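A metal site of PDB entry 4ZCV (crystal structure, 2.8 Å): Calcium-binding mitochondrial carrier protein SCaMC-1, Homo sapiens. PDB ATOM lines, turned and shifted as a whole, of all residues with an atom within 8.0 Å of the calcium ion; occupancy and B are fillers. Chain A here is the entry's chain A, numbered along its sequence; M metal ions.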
ATOM      1  N   VAL A  29      -0.021  13.180  25.823  1.00  0.00           N
ATOM      2  CA  VAL A  29      -0.224  14.107  24.711  1.00  0.00           C
ATOM      3  C   VAL A  29       0.573  13.656  23.487  1.00  0.00           C
ATOM      4  O   VAL A  29       1.515  12.878  23.609  1.00  0.00           O
ATOM      5  CB  VAL A  29       0.188  15.561  25.047  1.00  0.00           C
ATOM      6  CG1 VAL A  29      -0.657  16.104  26.195  1.00  0.00           C
ATOM      7  CG2 VAL A  29       1.667  15.637  25.375  1.00  0.00           C
ATOM      8  N   VAL A  30       0.156  14.127  22.332  1.00  0.00           N
ATOM      9  CA  VAL A  30       0.857  13.854  21.090  1.00  0.00           C
ATOM     10  C   VAL A  30       1.509  15.132  20.574  1.00  0.00           C
ATOM     11  O   VAL A  30       0.811  16.112  20.313  1.00  0.00           O
ATOM     12  CB  VAL A  30      -0.104  13.292  20.006  1.00  0.00           C
ATOM     13  CG1 VAL A  30       0.573  13.290  18.643  1.00  0.00           C
ATOM     14  CG2 VAL A  30      -0.571  11.896  20.382  1.00  0.00           C
ATOM     15  N   PHE A  55      -2.707  19.240  13.041  1.00  0.00           N
ATOM     16  CA  PHE A  55      -2.296  19.681  14.370  1.00  0.00           C
ATOM     17  C   PHE A  55      -2.884  21.046  14.720  1.00  0.00           C
ATOM     18  O   PHE A  55      -3.388  21.251  15.818  1.00  0.00           O
ATOM     19  CB  PHE A  55      -0.769  19.710  14.459  1.00  0.00           C
ATOM     20  CG  PHE A  55      -0.228  19.314  15.803  1.00  0.00           C
ATOM     21  CD1 PHE A  55      -0.189  20.223  16.839  1.00  0.00           C
ATOM     22  CD2 PHE A  55       0.226  18.021  16.022  1.00  0.00           C
ATOM     23  CE1 PHE A  55       0.308  19.859  18.086  1.00  0.00           C
ATOM     24  CE2 PHE A  55       0.721  17.646  17.256  1.00  0.00           C
ATOM     25  CZ  PHE A  55       0.764  18.564  18.292  1.00  0.00           C
ATOM     26  N   GLY A  58      -6.576  20.853  15.316  1.00  0.00           N
ATOM     27  CA  GLY A  58      -6.853  20.127  16.546  1.00  0.00           C
ATOM     28  C   GLY A  58      -6.432  20.812  17.835  1.00  0.00           C
ATOM     29  O   GLY A  58      -7.155  20.768  18.823  1.00  0.00           O
ATOM     30  N   ASP A  59      -5.254  21.430  17.835  1.00  0.00           N
ATOM     31  CA  ASP A  59      -4.726  22.053  19.038  1.00  0.00           C
ATOM     32  C   ASP A  59      -5.521  23.294  19.430  1.00  0.00           C
ATOM     33  O   ASP A  59      -5.120  24.422  19.148  1.00  0.00           O
ATOM     34  CB  ASP A  59      -3.248  22.419  18.859  1.00  0.00           C
ATOM     35  CG  ASP A  59      -2.588  22.893  20.140  1.00  0.00           C
ATOM     36  OD1 ASP A  59      -3.101  22.565  21.227  1.00  0.00           O
ATOM     37  OD2 ASP A  59      -1.549  23.573  20.064  1.00  0.00           O
ATOM     38  N   VAL A  60      -6.660  23.068  20.087  1.00  0.00           N
ATOM     39  CA  VAL A  60      -7.597  24.134  20.429  1.00  0.00           C
ATOM     40  C   VAL A  60      -7.046  25.104  21.480  1.00  0.00           C
ATOM     41  O   VAL A  60      -7.170  26.320  21.322  1.00  0.00           O
ATOM     42  CB  VAL A  60      -8.925  23.549  20.935  1.00  0.00           C
ATOM     43  CG1 VAL A  60      -9.847  24.647  21.448  1.00  0.00           C
ATOM     44  CG2 VAL A  60      -9.602  22.749  19.833  1.00  0.00           C
ATOM     45  N   ASN A  61      -6.422  24.582  22.526  1.00  0.00           N
ATOM     46  CA  ASN A  61      -5.895  25.440  23.594  1.00  0.00           C
ATOM     47  C   ASN A  61      -4.548  26.042  23.203  1.00  0.00           C
ATOM     48  O   ASN A  61      -3.945  26.790  23.971  1.00  0.00           O
ATOM     49  CB  ASN A  61      -5.757  24.659  24.889  1.00  0.00           C
ATOM     50  CG  ASN A  61      -4.753  23.530  24.779  1.00  0.00           C
ATOM     51  OD1 ASN A  61      -4.506  23.021  23.686  1.00  0.00           O
ATOM     52  ND2 ASN A  61      -4.173  23.138  25.904  1.00  0.00           N
ATOM     53  N   LYS A  62      -4.083  25.695  22.000  1.00  0.00           N
ATOM     54  CA  LYS A  62      -2.876  26.253  21.416  1.00  0.00           C
ATOM     55  C   LYS A  62      -1.656  26.198  22.341  1.00  0.00           C
ATOM     56  O   LYS A  62      -1.012  27.213  22.616  1.00  0.00           O
ATOM     57  CB  LYS A  62      -3.142  27.685  20.962  1.00  0.00           C
ATOM     58  CG  LYS A  62      -4.223  27.749  19.890  1.00  0.00           C
ATOM     59  CD  LYS A  62      -4.494  29.160  19.409  1.00  0.00           C
ATOM     60  CE  LYS A  62      -5.417  29.143  18.189  1.00  0.00           C
ATOM     61  NZ  LYS A  62      -5.749  30.519  17.711  1.00  0.00           N
ATOM     62  N   ASP A  63      -1.353  24.998  22.831  1.00  0.00           N
ATOM     63  CA  ASP A  63      -0.183  24.784  23.666  1.00  0.00           C
ATOM     64  C   ASP A  63       0.863  23.962  22.916  1.00  0.00           C
ATOM     65  O   ASP A  63       1.862  23.537  23.501  1.00  0.00           O
ATOM     66  CB  ASP A  63      -0.581  24.094  24.984  1.00  0.00           C
ATOM     67  CG  ASP A  63      -1.122  22.704  24.773  1.00  0.00           C
ATOM     68  OD1 ASP A  63      -1.541  22.367  23.639  1.00  0.00           O
ATOM     69  OD2 ASP A  63      -1.171  21.947  25.766  1.00  0.00           O
ATOM     70  N   GLY A  64       0.625  23.736  21.630  1.00  0.00           N
ATOM     71  CA  GLY A  64       1.559  23.007  20.796  1.00  0.00           C
ATOM     72  C   GLY A  64       1.484  21.503  21.001  1.00  0.00           C
ATOM     73  O   GLY A  64       2.330  20.755  20.509  1.00  0.00           O
ATOM     74  N   LYS A  65       0.474  21.059  21.730  1.00  0.00           N
ATOM     75  CA  LYS A  65       0.312  19.640  22.029  1.00  0.00           C
ATOM     76  C   LYS A  65      -1.096  19.192  21.688  1.00  0.00           C
ATOM     77  O   LYS A  65      -2.028  20.003  21.680  1.00  0.00           O
ATOM     78  CB  LYS A  65       0.601  19.353  23.504  1.00  0.00           C
ATOM     79  CG  LYS A  65       1.952  19.861  24.009  1.00  0.00           C
ATOM     80  CD  LYS A  65       2.096  19.633  25.507  1.00  0.00           C
ATOM     81  CE  LYS A  65       3.102  20.598  26.112  1.00  0.00           C
ATOM     82  NZ  LYS A  65       3.160  20.507  27.597  1.00  0.00           N
ATOM     83  N   LEU A  66      -1.255  17.908  21.368  1.00  0.00           N
ATOM     84  CA  LEU A  66      -2.579  17.339  21.169  1.00  0.00           C
ATOM     85  C   LEU A  66      -2.907  16.363  22.306  1.00  0.00           C
ATOM     86  O   LEU A  66      -2.374  15.261  22.364  1.00  0.00           O
ATOM     87  CB  LEU A  66      -2.660  16.613  19.825  1.00  0.00           C
ATOM     88  CG  LEU A  66      -2.758  17.465  18.564  1.00  0.00           C
ATOM     89  CD1 LEU A  66      -2.833  16.580  17.325  1.00  0.00           C
ATOM     90  CD2 LEU A  66      -3.961  18.394  18.640  1.00  0.00           C
ATOM     91  N   ASP A  67      -3.789  16.781  23.219  1.00  0.00           N
ATOM     92  CA  ASP A  67      -4.240  15.858  24.254  1.00  0.00           C
ATOM     93  C   ASP A  67      -5.300  14.945  23.650  1.00  0.00           C
ATOM     94  O   ASP A  67      -5.727  15.150  22.517  1.00  0.00           O
ATOM     95  CB  ASP A  67      -4.786  16.605  25.485  1.00  0.00           C
ATOM     96  CG  ASP A  67      -5.851  17.625  25.125  1.00  0.00           C
ATOM     97  OD1 ASP A  67      -6.795  17.272  24.401  1.00  0.00           O
ATOM     98  OD2 ASP A  67      -5.748  18.785  25.588  1.00  0.00           O
ATOM     99  N   PHE A  68      -5.735  13.946  24.408  1.00  0.00           N
ATOM    100  CA  PHE A  68      -6.619  12.927  23.855  1.00  0.00           C
ATOM    101  C   PHE A  68      -7.985  13.482  23.455  1.00  0.00           C
ATOM    102  O   PHE A  68      -8.615  12.972  22.534  1.00  0.00           O
ATOM    103  CB  PHE A  68      -6.796  11.782  24.846  1.00  0.00           C
ATOM    104  CG  PHE A  68      -7.813  10.773  24.417  1.00  0.00           C
ATOM    105  CD1 PHE A  68      -7.606  10.022  23.275  1.00  0.00           C
ATOM    106  CD2 PHE A  68      -8.965  10.579  25.140  1.00  0.00           C
ATOM    107  CE1 PHE A  68      -8.540   9.082  22.864  1.00  0.00           C
ATOM    108  CE2 PHE A  68      -9.909   9.645  24.748  1.00  0.00           C
ATOM    109  CZ  PHE A  68      -9.691   8.899  23.614  1.00  0.00           C
ATOM    110  N   GLU A  69      -8.428  14.540  24.119  1.00  0.00           N
ATOM    111  CA  GLU A  69      -9.751  15.077  23.857  1.00  0.00           C
ATOM    112  C   GLU A  69      -9.753  15.980  22.625  1.00  0.00           C
ATOM    113  O   GLU A  69     -10.757  16.025  21.889  1.00  0.00           O
ATOM    114  CB  GLU A  69     -10.297  15.824  25.089  1.00  0.00           C
ATOM    115  CG  GLU A  69      -9.269  16.513  25.973  1.00  0.00           C
ATOM    116  CD  GLU A  69      -8.613  15.584  26.984  1.00  0.00           C
ATOM    117  OE1 GLU A  69      -8.361  14.404  26.645  1.00  0.00           O
ATOM    118  OE2 GLU A  69      -8.386  16.028  28.137  1.00  0.00           O
ATOM    119  N   GLU A  70      -8.638  16.657  22.366  1.00  0.00           N
ATOM    120  CA  GLU A  70      -8.474  17.435  21.149  1.00  0.00           C
ATOM    121  C   GLU A  70      -8.390  16.498  19.954  1.00  0.00           C
ATOM    122  O   GLU A  70      -9.001  16.727  18.907  1.00  0.00           O
ATOM    123  CB  GLU A  70      -7.224  18.302  21.218  1.00  0.00           C
ATOM    124  CG  GLU A  70      -7.276  19.498  22.179  1.00  0.00           C
ATOM    125  CD  GLU A  70      -5.907  20.145  22.362  1.00  0.00           C
ATOM    126  OE1 GLU A  70      -4.880  19.447  22.198  1.00  0.00           O
ATOM    127  OE2 GLU A  70      -5.853  21.360  22.654  1.00  0.00           O
ATOM    128  N   PHE A  71      -7.624  15.420  20.142  1.00  0.00           N
ATOM    129  CA  PHE A  71      -7.411  14.397  19.133  1.00  0.00           C
ATOM    130  C   PHE A  71      -8.734  13.740  18.735  1.00  0.00           C
ATOM    131  O   PHE A  71      -9.107  13.684  17.561  1.00  0.00           O
ATOM    132  CB  PHE A  71      -6.403  13.370  19.673  1.00  0.00           C
ATOM    133  CG  PHE A  71      -6.024  12.291  18.701  1.00  0.00           C
ATOM    134  CD1 PHE A  71      -5.090  12.538  17.704  1.00  0.00           C
ATOM    135  CD2 PHE A  71      -6.559  11.025  18.829  1.00  0.00           C
ATOM    136  CE1 PHE A  71      -4.731  11.529  16.814  1.00  0.00           C
ATOM    137  CE2 PHE A  71      -6.201  10.017  17.953  1.00  0.00           C
ATOM    138  CZ  PHE A  71      -5.284  10.274  16.945  1.00  0.00           C
HETATM  139 CA    CA M   1      -3.453  21.104  23.070  1.00  0.00          CA
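OD1 of Asn 61 binds the calcium ion (2.3 Å). The calcium ion is bound by the backbone carbonyl oxygen (O) of Lys 65 (2.3 Å). OE1 of Glu 70 is bound to the calcium ion. The side-chain carboxylate (OD1) of Asp 63 binds the calcium ion (2.4 Å). OD1 of Asp 59 is bound to the calcium ion (2.4 Å). OE2 of Glu 70 binds the calcium ion, 2.4 Å away.
The backbone NH of Glu 70 lies within hydrogen-bond range of the side-chain carboxylate of Asp 67 (2.8 Å). The backbone NH (N) of Val 60 lies close to the side-chain carboxylate (OE2) of Glu 70. N of Lys 62 lies close to OD1 of Asp 59 (3.4 Å). The backbone NH of Gly 64 sits at hydrogen-bond distance from the side-chain carboxylate of Asp 59, at 2.7 Å.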
